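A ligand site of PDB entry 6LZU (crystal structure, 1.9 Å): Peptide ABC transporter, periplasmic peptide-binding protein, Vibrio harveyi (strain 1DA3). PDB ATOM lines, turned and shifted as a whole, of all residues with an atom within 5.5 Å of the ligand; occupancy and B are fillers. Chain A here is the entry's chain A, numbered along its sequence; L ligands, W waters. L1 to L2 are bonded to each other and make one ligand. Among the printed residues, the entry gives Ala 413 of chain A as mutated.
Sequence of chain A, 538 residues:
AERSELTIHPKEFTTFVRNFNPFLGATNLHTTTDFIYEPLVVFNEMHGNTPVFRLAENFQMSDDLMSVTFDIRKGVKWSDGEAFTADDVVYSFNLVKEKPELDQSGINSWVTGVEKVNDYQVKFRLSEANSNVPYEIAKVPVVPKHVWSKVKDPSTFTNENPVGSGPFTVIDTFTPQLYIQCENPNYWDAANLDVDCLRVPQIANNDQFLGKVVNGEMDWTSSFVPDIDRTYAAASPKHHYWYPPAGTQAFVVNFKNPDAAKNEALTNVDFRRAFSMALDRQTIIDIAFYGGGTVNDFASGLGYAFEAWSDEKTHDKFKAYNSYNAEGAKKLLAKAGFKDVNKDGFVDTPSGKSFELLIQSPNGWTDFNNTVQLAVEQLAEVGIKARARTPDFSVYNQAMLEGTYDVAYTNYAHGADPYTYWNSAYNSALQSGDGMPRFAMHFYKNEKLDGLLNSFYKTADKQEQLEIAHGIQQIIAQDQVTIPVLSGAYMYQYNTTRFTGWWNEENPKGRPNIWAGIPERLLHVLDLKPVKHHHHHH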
ATOM      1  N   HIS A   9     -20.112   2.025  33.930  1.00  0.00           N
ATOM      2  CA  HIS A   9     -20.617   2.817  32.811  1.00  0.00           C
ATOM      3  C   HIS A   9     -19.959   2.389  31.496  1.00  0.00           C
ATOM      4  O   HIS A   9     -18.970   2.978  31.061  1.00  0.00           O
ATOM      5  CB  HIS A   9     -20.402   4.315  33.095  1.00  0.00           C
ATOM      6  CG  HIS A   9     -20.865   5.222  31.986  1.00  0.00           C
ATOM      7  ND1 HIS A   9     -22.007   4.976  31.256  1.00  0.00           N
ATOM      8  CD2 HIS A   9     -20.336   6.362  31.497  1.00  0.00           C
ATOM      9  CE1 HIS A   9     -22.148   5.928  30.349  1.00  0.00           C
ATOM     10  NE2 HIS A   9     -21.162   6.793  30.483  1.00  0.00           N
ATOM     11  N   PRO A  10     -20.484   1.335  30.859  1.00  0.00           N
ATOM     12  CA  PRO A  10     -19.875   0.828  29.618  1.00  0.00           C
ATOM     13  C   PRO A  10     -20.187   1.631  28.337  1.00  0.00           C
ATOM     14  O   PRO A  10     -19.388   1.635  27.400  1.00  0.00           O
ATOM     15  CB  PRO A  10     -20.444  -0.586  29.503  1.00  0.00           C
ATOM     16  CG  PRO A  10     -21.751  -0.538  30.264  1.00  0.00           C
ATOM     17  CD  PRO A  10     -21.500   0.420  31.412  1.00  0.00           C
ATOM     18  N   LYS A  11     -21.323   2.313  28.292  1.00  0.00           N
ATOM     19  CA  LYS A  11     -21.823   2.889  27.036  1.00  0.00           C
ATOM     20  C   LYS A  11     -22.829   3.990  27.318  1.00  0.00           C
ATOM     21  O   LYS A  11     -23.673   3.840  28.196  1.00  0.00           O
ATOM     22  CB  LYS A  11     -22.484   1.785  26.198  1.00  0.00           C
ATOM     23  CG  LYS A  11     -23.144   2.248  24.897  1.00  0.00           C
ATOM     24  CD  LYS A  11     -22.117   2.749  23.898  1.00  0.00           C
ATOM     25  CE  LYS A  11     -22.618   2.707  22.450  1.00  0.00           C
ATOM     26  NZ  LYS A  11     -24.053   2.988  22.349  1.00  0.00           N
ATOM     27  N   GLU A  12     -22.770   5.072  26.553  1.00  0.00           N
ATOM     28  CA  GLU A  12     -23.792   6.121  26.656  1.00  0.00           C
ATOM     29  C   GLU A  12     -25.138   5.664  26.084  1.00  0.00           C
ATOM     30  O   GLU A  12     -25.182   4.948  25.083  1.00  0.00           O
ATOM     31  CB  GLU A  12     -23.343   7.391  25.919  1.00  0.00           C
ATOM     32  CG  GLU A  12     -21.925   7.863  26.271  1.00  0.00           C
ATOM     33  CD  GLU A  12     -20.824   7.307  25.348  1.00  0.00           C
ATOM     34  OE1 GLU A  12     -20.984   6.210  24.755  1.00  0.00           O
ATOM     35  OE2 GLU A  12     -19.786   7.979  25.222  1.00  0.00           O
ATOM     36  N   ASN A 206     -20.420  13.177  27.757  1.00  0.00           N
ATOM     37  CA  ASN A 206     -19.302  13.369  28.671  1.00  0.00           C
ATOM     38  C   ASN A 206     -19.563  14.435  29.734  1.00  0.00           C
ATOM     39  O   ASN A 206     -19.038  14.340  30.840  1.00  0.00           O
ATOM     40  CB  ASN A 206     -18.025  13.724  27.891  1.00  0.00           C
ATOM     41  CG  ASN A 206     -17.388  12.511  27.204  1.00  0.00           C
ATOM     42  OD1 ASN A 206     -17.823  11.376  27.391  1.00  0.00           O
ATOM     43  ND2 ASN A 206     -16.363  12.759  26.403  1.00  0.00           N
ATOM     44  N   SER A 222     -14.708   4.321  32.106  1.00  0.00           N
ATOM     45  CA  SER A 222     -13.682   4.418  31.059  1.00  0.00           C
ATOM     46  C   SER A 222     -13.997   5.567  30.098  1.00  0.00           C
ATOM     47  O   SER A 222     -13.748   5.467  28.904  1.00  0.00           O
ATOM     48  CB  SER A 222     -13.577   3.082  30.275  1.00  0.00           C
ATOM     49  OG  SER A 222     -13.019   2.030  31.078  1.00  0.00           O
ATOM     50  N   SER A 223     -14.541   6.664  30.620  1.00  0.00           N
ATOM     51  CA  SER A 223     -14.927   7.802  29.779  1.00  0.00           C
ATOM     52  C   SER A 223     -13.807   8.810  29.670  1.00  0.00           C
ATOM     53  O   SER A 223     -12.867   8.787  30.467  1.00  0.00           O
ATOM     54  CB  SER A 223     -16.180   8.503  30.317  1.00  0.00           C
ATOM     55  OG  SER A 223     -17.284   7.617  30.354  1.00  0.00           O
ATOM     56  N   PHE A 224     -13.891   9.697  28.671  1.00  0.00           N
ATOM     57  CA  PHE A 224     -12.979  10.810  28.656  1.00  0.00           C
ATOM     58  C   PHE A 224     -13.313  11.775  29.812  1.00  0.00           C
ATOM     59  O   PHE A 224     -14.486  12.059  30.064  1.00  0.00           O
ATOM     60  CB  PHE A 224     -13.037  11.570  27.328  1.00  0.00           C
ATOM     61  CG  PHE A 224     -12.223  12.844  27.347  1.00  0.00           C
ATOM     62  CD1 PHE A 224     -10.834  12.784  27.281  1.00  0.00           C
ATOM     63  CD2 PHE A 224     -12.846  14.076  27.459  1.00  0.00           C
ATOM     64  CE1 PHE A 224     -10.083  13.943  27.317  1.00  0.00           C
ATOM     65  CE2 PHE A 224     -12.113  15.234  27.492  1.00  0.00           C
ATOM     66  CZ  PHE A 224     -10.714  15.170  27.405  1.00  0.00           C
ATOM     67  N   GLN A 249      -5.845   6.710  16.271  1.00  0.00           N
ATOM     68  CA  GLN A 249      -6.980   7.546  15.909  1.00  0.00           C
ATOM     69  C   GLN A 249      -6.622   8.292  14.631  1.00  0.00           C
ATOM     70  O   GLN A 249      -5.474   8.705  14.447  1.00  0.00           O
ATOM     71  CB  GLN A 249      -7.342   8.529  17.040  1.00  0.00           C
ATOM     72  CG  GLN A 249      -7.684   7.831  18.354  1.00  0.00           C
ATOM     73  CD  GLN A 249      -8.076   8.774  19.475  1.00  0.00           C
ATOM     74  OE1 GLN A 249      -8.240   9.972  19.279  1.00  0.00           O
ATOM     75  NE2 GLN A 249      -8.230   8.214  20.673  1.00  0.00           N
ATOM     76  N   PHE A 289      -6.973  16.414  24.344  1.00  0.00           N
ATOM     77  CA  PHE A 289      -6.772  15.266  25.227  1.00  0.00           C
ATOM     78  C   PHE A 289      -5.947  15.568  26.474  1.00  0.00           C
ATOM     79  O   PHE A 289      -5.573  14.650  27.216  1.00  0.00           O
ATOM     80  CB  PHE A 289      -6.099  14.118  24.444  1.00  0.00           C
ATOM     81  CG  PHE A 289      -6.947  13.580  23.314  1.00  0.00           C
ATOM     82  CD1 PHE A 289      -6.881  14.148  22.062  1.00  0.00           C
ATOM     83  CD2 PHE A 289      -7.789  12.499  23.500  1.00  0.00           C
ATOM     84  CE1 PHE A 289      -7.632  13.653  21.014  1.00  0.00           C
ATOM     85  CE2 PHE A 289      -8.557  12.003  22.450  1.00  0.00           C
ATOM     86  CZ  PHE A 289      -8.476  12.584  21.207  1.00  0.00           C
ATOM     87  N   GLY A 364     -21.361  13.741  22.011  1.00  0.00           N
ATOM     88  CA  GLY A 364     -21.033  13.447  23.389  1.00  0.00           C
ATOM     89  C   GLY A 364     -19.594  13.007  23.608  1.00  0.00           C
ATOM     90  O   GLY A 364     -19.124  12.978  24.740  1.00  0.00           O
ATOM     91  N   TRP A 365     -18.905  12.654  22.523  1.00  0.00           N
ATOM     92  CA  TRP A 365     -17.511  12.223  22.636  1.00  0.00           C
ATOM     93  C   TRP A 365     -16.621  13.458  22.523  1.00  0.00           C
ATOM     94  O   TRP A 365     -15.994  13.697  21.496  1.00  0.00           O
ATOM     95  CB  TRP A 365     -17.117  11.208  21.545  1.00  0.00           C
ATOM     96  CG  TRP A 365     -17.829   9.885  21.539  1.00  0.00           C
ATOM     97  CD1 TRP A 365     -19.032   9.578  22.114  1.00  0.00           C
ATOM     98  CD2 TRP A 365     -17.368   8.680  20.910  1.00  0.00           C
ATOM     99  NE1 TRP A 365     -19.350   8.267  21.877  1.00  0.00           N
ATOM    100  CE2 TRP A 365     -18.346   7.688  21.149  1.00  0.00           C
ATOM    101  CE3 TRP A 365     -16.233   8.350  20.177  1.00  0.00           C
ATOM    102  CZ2 TRP A 365     -18.227   6.375  20.673  1.00  0.00           C
ATOM    103  CZ3 TRP A 365     -16.097   7.038  19.703  1.00  0.00           C
ATOM    104  CH2 TRP A 365     -17.091   6.078  19.954  1.00  0.00           C
ATOM    105  N   THR A 366     -16.569  14.247  23.602  1.00  0.00           N
ATOM    106  CA  THR A 366     -16.122  15.627  23.489  1.00  0.00           C
ATOM    107  C   THR A 366     -14.648  15.762  23.158  1.00  0.00           C
ATOM    108  O   THR A 366     -14.241  16.737  22.536  1.00  0.00           O
ATOM    109  CB  THR A 366     -16.427  16.394  24.782  1.00  0.00           C
ATOM    110  OG1 THR A 366     -15.813  15.712  25.889  1.00  0.00           O
ATOM    111  CG2 THR A 366     -17.941  16.473  25.004  1.00  0.00           C
ATOM    112  N   ASP A 367     -13.834  14.799  23.562  1.00  0.00           N
ATOM    113  CA  ASP A 367     -12.438  14.811  23.153  1.00  0.00           C
ATOM    114  C   ASP A 367     -12.295  14.719  21.612  1.00  0.00           C
ATOM    115  O   ASP A 367     -11.431  15.388  21.038  1.00  0.00           O
ATOM    116  CB  ASP A 367     -11.628  13.696  23.838  1.00  0.00           C
ATOM    117  CG  ASP A 367     -12.284  12.322  23.747  1.00  0.00           C
ATOM    118  OD1 ASP A 367     -13.515  12.207  23.580  1.00  0.00           O
ATOM    119  OD2 ASP A 367     -11.543  11.333  23.894  1.00  0.00           O
ATOM    120  N   PHE A 368     -13.124  13.915  20.953  1.00  0.00           N
ATOM    121  CA  PHE A 368     -13.084  13.822  19.493  1.00  0.00           C
ATOM    122  C   PHE A 368     -13.751  15.048  18.850  1.00  0.00           C
ATOM    123  O   PHE A 368     -13.320  15.507  17.795  1.00  0.00           O
ATOM    124  CB  PHE A 368     -13.768  12.567  18.961  1.00  0.00           C
ATOM    125  CG  PHE A 368     -13.058  11.264  19.247  1.00  0.00           C
ATOM    126  CD1 PHE A 368     -12.010  11.184  20.166  1.00  0.00           C
ATOM    127  CD2 PHE A 368     -13.462  10.093  18.605  1.00  0.00           C
ATOM    128  CE1 PHE A 368     -11.385   9.955  20.425  1.00  0.00           C
ATOM    129  CE2 PHE A 368     -12.848   8.871  18.863  1.00  0.00           C
ATOM    130  CZ  PHE A 368     -11.789   8.808  19.768  1.00  0.00           C
ATOM    131  N   ASN A 411     -11.503   6.342  16.375  1.00  0.00           N
ATOM    132  CA  ASN A 411     -10.507   5.451  16.921  1.00  0.00           C
ATOM    133  C   ASN A 411     -10.697   4.069  16.338  1.00  0.00           C
ATOM    134  O   ASN A 411     -11.619   3.848  15.562  1.00  0.00           O
ATOM    135  CB  ASN A 411     -10.555   5.381  18.455  1.00  0.00           C
ATOM    136  CG  ASN A 411     -11.958   5.193  19.010  1.00  0.00           C
ATOM    137  OD1 ASN A 411     -12.950   5.301  18.297  1.00  0.00           O
ATOM    138  ND2 ASN A 411     -12.037   4.922  20.310  1.00  0.00           N
ATOM    139  N   TYR A 412      -9.823   3.152  16.748  1.00  0.00           N
ATOM    140  CA  TYR A 412      -9.796   1.790  16.248  1.00  0.00           C
ATOM    141  C   TYR A 412      -9.507   0.833  17.387  1.00  0.00           C
ATOM    142  O   TYR A 412      -8.912   1.236  18.383  1.00  0.00           O
ATOM    143  CB  TYR A 412      -8.709   1.584  15.194  1.00  0.00           C
ATOM    144  CG  TYR A 412      -8.831   2.390  13.928  1.00  0.00           C
ATOM    145  CD1 TYR A 412      -8.288   3.655  13.830  1.00  0.00           C
ATOM    146  CD2 TYR A 412      -9.459   1.862  12.810  1.00  0.00           C
ATOM    147  CE1 TYR A 412      -8.375   4.378  12.671  1.00  0.00           C
ATOM    148  CE2 TYR A 412      -9.568   2.574  11.649  1.00  0.00           C
ATOM    149  CZ  TYR A 412      -9.022   3.824  11.579  1.00  0.00           C
ATOM    150  OH  TYR A 412      -9.103   4.509  10.400  1.00  0.00           O
ATOM    151  N   ALA A 413      -9.882  -0.424  17.199  1.00  0.00           N
ATOM    152  CA  ALA A 413      -9.408  -1.489  18.078  1.00  0.00           C
ATOM    153  C   ALA A 413      -7.889  -1.567  18.020  1.00  0.00           C
ATOM    154  O   ALA A 413      -7.268  -1.267  16.998  1.00  0.00           O
ATOM    155  CB  ALA A 413     -10.032  -2.821  17.691  1.00  0.00           C
ATOM    156  N   ARG A 438     -17.800   0.467  11.561  1.00  0.00           N
ATOM    157  CA  ARG A 438     -17.433   1.604  10.717  1.00  0.00           C
ATOM    158  C   ARG A 438     -16.024   1.579  10.168  1.00  0.00           C
ATOM    159  O   ARG A 438     -15.709   2.333   9.241  1.00  0.00           O
ATOM    160  CB  ARG A 438     -17.601   2.907  11.515  1.00  0.00           C
ATOM    161  CG  ARG A 438     -16.658   3.025  12.730  1.00  0.00           C
ATOM    162  CD  ARG A 438     -17.050   4.235  13.611  1.00  0.00           C
ATOM    163  NE  ARG A 438     -16.145   4.449  14.740  1.00  0.00           N
ATOM    164  CZ  ARG A 438     -16.188   3.757  15.884  1.00  0.00           C
ATOM    165  NH1 ARG A 438     -17.085   2.802  16.047  1.00  0.00           N
ATOM    166  NH2 ARG A 438     -15.320   4.013  16.851  1.00  0.00           N
ATOM    167  N   PHE A 439     -15.156   0.728  10.726  1.00  0.00           N
ATOM    168  CA  PHE A 439     -13.727   1.016  10.670  1.00  0.00           C
ATOM    169  C   PHE A 439     -13.130   0.953   9.276  1.00  0.00           C
ATOM    170  O   PHE A 439     -12.200   1.697   8.972  1.00  0.00           O
ATOM    171  CB  PHE A 439     -12.955   0.075  11.611  1.00  0.00           C
ATOM    172  CG  PHE A 439     -13.414   0.161  13.014  1.00  0.00           C
ATOM    173  CD1 PHE A 439     -13.153   1.284  13.768  1.00  0.00           C
ATOM    174  CD2 PHE A 439     -14.184  -0.853  13.578  1.00  0.00           C
ATOM    175  CE1 PHE A 439     -13.602   1.392  15.072  1.00  0.00           C
ATOM    176  CE2 PHE A 439     -14.645  -0.749  14.888  1.00  0.00           C
ATOM    177  CZ  PHE A 439     -14.360   0.383  15.631  1.00  0.00           C
ATOM    178  N   MET A 491      -8.698   4.891  28.585  1.00  0.00           N
ATOM    179  CA  MET A 491      -9.190   5.695  29.711  1.00  0.00           C
ATOM    180  C   MET A 491      -9.836   4.771  30.744  1.00  0.00           C
ATOM    181  O   MET A 491     -10.640   3.914  30.403  1.00  0.00           O
ATOM    182  CB  MET A 491     -10.209   6.747  29.252  1.00  0.00           C
ATOM    183  CG  MET A 491      -9.734   7.671  28.141  1.00  0.00           C
ATOM    184  SD  MET A 491     -10.294   7.079  26.541  1.00  0.00           S
ATOM    185  CE  MET A 491     -12.078   7.252  26.650  1.00  0.00           C
ATOM    186  N   TRP A 515     -15.599  -1.087  28.943  1.00  0.00           N
ATOM    187  CA  TRP A 515     -16.276  -1.183  27.639  1.00  0.00           C
ATOM    188  C   TRP A 515     -16.634  -2.625  27.243  1.00  0.00           C
ATOM    189  O   TRP A 515     -15.884  -3.557  27.525  1.00  0.00           O
ATOM    190  CB  TRP A 515     -15.387  -0.607  26.522  1.00  0.00           C
ATOM    191  CG  TRP A 515     -15.019   0.841  26.683  1.00  0.00           C
ATOM    192  CD1 TRP A 515     -15.785   1.846  27.224  1.00  0.00           C
ATOM    193  CD2 TRP A 515     -13.776   1.428  26.320  1.00  0.00           C
ATOM    194  NE1 TRP A 515     -15.077   3.021  27.218  1.00  0.00           N
ATOM    195  CE2 TRP A 515     -13.843   2.798  26.659  1.00  0.00           C
ATOM    196  CE3 TRP A 515     -12.595   0.934  25.754  1.00  0.00           C
ATOM    197  CZ2 TRP A 515     -12.771   3.675  26.448  1.00  0.00           C
ATOM    198  CZ3 TRP A 515     -11.543   1.801  25.526  1.00  0.00           C
ATOM    199  CH2 TRP A 515     -11.639   3.153  25.876  1.00  0.00           C
ATOM    200  N   ALA A 516     -17.766  -2.798  26.577  1.00  0.00           N
ATOM    201  CA  ALA A 516     -18.017  -4.045  25.877  1.00  0.00           C
ATOM    202  C   ALA A 516     -16.980  -4.183  24.758  1.00  0.00           C
ATOM    203  O   ALA A 516     -16.619  -3.192  24.109  1.00  0.00           O
ATOM    204  CB  ALA A 516     -19.453  -4.103  25.335  1.00  0.00           C
HETATM  205  C1  LIG L   1     -16.195   1.697  22.319  1.00  0.00           C
HETATM  206  C2  LIG L   1     -15.261   2.766  21.759  1.00  0.00           C
HETATM  207  C3  LIG L   1     -14.909   3.747  22.876  1.00  0.00           C
HETATM  208  C4  LIG L   1     -16.187   4.294  23.530  1.00  0.00           C
HETATM  209  C5  LIG L   1     -17.114   3.147  23.936  1.00  0.00           C
HETATM  210  C6  LIG L   1     -18.428   3.672  24.514  1.00  0.00           C
HETATM  211  C7  LIG L   1     -14.006   2.016  19.818  1.00  0.00           C
HETATM  212  C8  LIG L   1     -12.684   1.531  19.290  1.00  0.00           C
HETATM  213  N1  LIG L   1     -14.072   2.177  21.146  1.00  0.00           N
HETATM  214  O1  LIG L   1     -16.557   0.751  21.314  1.00  0.00           O
HETATM  215  O2  LIG L   1     -14.131   4.803  22.312  1.00  0.00           O
HETATM  216  O3  LIG L   1     -15.893   5.051  24.702  1.00  0.00           O
HETATM  217  O4  LIG L   1     -17.390   2.319  22.810  1.00  0.00           O
HETATM  218  O5  LIG L   1     -19.055   4.529  23.543  1.00  0.00           O
HETATM  219  O6  LIG L   1     -14.957   2.274  19.093  1.00  0.00           O
HETATM  220  C1  LG2 L   2     -16.021   6.470  24.541  1.00  0.00           C
HETATM  221  C2  LG2 L   2     -16.237   7.123  25.903  1.00  0.00           C
HETATM  222  C3  LG2 L   2     -16.229   8.638  25.706  1.00  0.00           C
HETATM  223  C4  LG2 L   2     -15.030   9.154  24.920  1.00  0.00           C
HETATM  224  C5  LG2 L   2     -14.891   8.370  23.615  1.00  0.00           C
HETATM  225  C6  LG2 L   2     -13.650   8.770  22.801  1.00  0.00           C
HETATM  226  C7  LG2 L   2     -17.654   5.870  27.521  1.00  0.00           C
HETATM  227  C8  LG2 L   2     -19.061   5.630  27.991  1.00  0.00           C
HETATM  228  N1  LG2 L   2     -17.515   6.709  26.493  1.00  0.00           N
HETATM  229  O1  LG2 L   2     -16.294   9.300  26.973  1.00  0.00           O
HETATM  230  O2  LG2 L   2     -15.257  10.545  24.634  1.00  0.00           O
HETATM  231  O3  LG2 L   2     -14.813   6.973  23.934  1.00  0.00           O
HETATM  232  O4  LG2 L   2     -12.462   8.833  23.612  1.00  0.00           O
HETATM  233  O5  LG2 L   2     -16.713   5.302  28.053  1.00  0.00           O
HETATM  234  O   HOH W   1     -17.043   5.032  30.926  1.00  0.00           O
HETATM  235  O   HOH W   2     -17.605  -0.902  23.341  1.00  0.00           O
HETATM  236  O   HOH W   3     -19.349   2.932  21.235  1.00  0.00           O
HETATM  237  O   HOH W   4     -17.612   1.654  18.844  1.00  0.00           O
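NH2 of Arg 438 is in hydrogen-bond range of O6 of LIG L1 (2.9 Å).
The backbone NH of Phe 224 is in hydrogen-bond range of an oxygen (O1) of LG2 L2 (3.0 Å).
The side-chain amide nitrogen (ND2) of Asn 411 sits at hydrogen-bond distance from an oxygen (O2) of LIG L1, at 2.9 Å.
OD1 of Asn 206 is in hydrogen-bond range of O1 of LG2 L2.
The side-chain carboxylate of Asp 367 sits at hydrogen-bond distance from an oxygen (O2) of LG2 L2.
O5 of LG2 L2 lies within hydrogen-bond range of OG of Ser 223 (3.3 Å).
An oxygen (O5) of LIG L1 sits at hydrogen-bond distance from the side-chain carboxylate of Glu 12 (2.8 Å).
The indole nitrogen of Trp 515 lies within hydrogen-bond range of an oxygen (O5) of LG2 L2, at 2.9 Å.
O of Met 491 lies close to OG of Ser 222.
The backbone carbonyl oxygen of Ser 222 sits close to the indole nitrogen of Trp 515, at 3.3 Å.
The backbone carbonyl oxygen (O) of Gly 364 sits close to the side-chain amide nitrogen (ND2) of Asn 206.
The side-chain amide nitrogen (ND2) of Asn 206 lies within hydrogen-bond range of the side-chain hydroxyl (OG1) of Thr 366 (3.0 Å).
The guanidinium group (NH2) of Arg 438 lies within hydrogen-bond range of the side-chain amide oxygen (OD1) of Asn 411 (3.1 Å).
The side-chain carboxylate (OE2) of Glu 12 is in hydrogen-bond range of the indole nitrogen (NE1) of Trp 365, 3.4 Å away.
The backbone carbonyl oxygen (O) of Ser 222 lies close to an oxygen (O5) of LG2 L2, 3.1 Å away.
Merely in contact with the ligand: His 9 (3.5 Å), Pro 10 (3.7 Å), Lys 11 (3.6 Å), Trp 365 (3.4 Å), Phe 368 (3.5 Å), Tyr 412 (3.8 Å), Phe 439 (3.99 Å) and Met 491 (3.4 Å).
Hydrophobic or aromatic side chains within 4 Å of the ligand: His 9, Phe 224, Trp 365, Phe 368, Phe 439, Met 491 and Trp 515.
Of the 23 residues printed, 17 come within 4 Å of the ligand.
The nearest printed residue that does not touch the ligand is Ala 413 (4.01 Å).
Water W4 bridges an oxygen (O6) of LIG L1 (2.7 Å) and the guanidinium group (NH1) of Arg 438 (3.1 Å).
Water W2 bridges the backbone carbonyl oxygen of Ala 516 (2.6 Å) and an oxygen (O1) of LIG L1 (2.8 Å).
Water W1 lies within hydrogen-bond range of OG of Ser 223 (2.7 Å), N of Ser 222 (2.7 Å), O of His 9 (2.8 Å) and O5 of LG2 L2 (2.9 Å).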
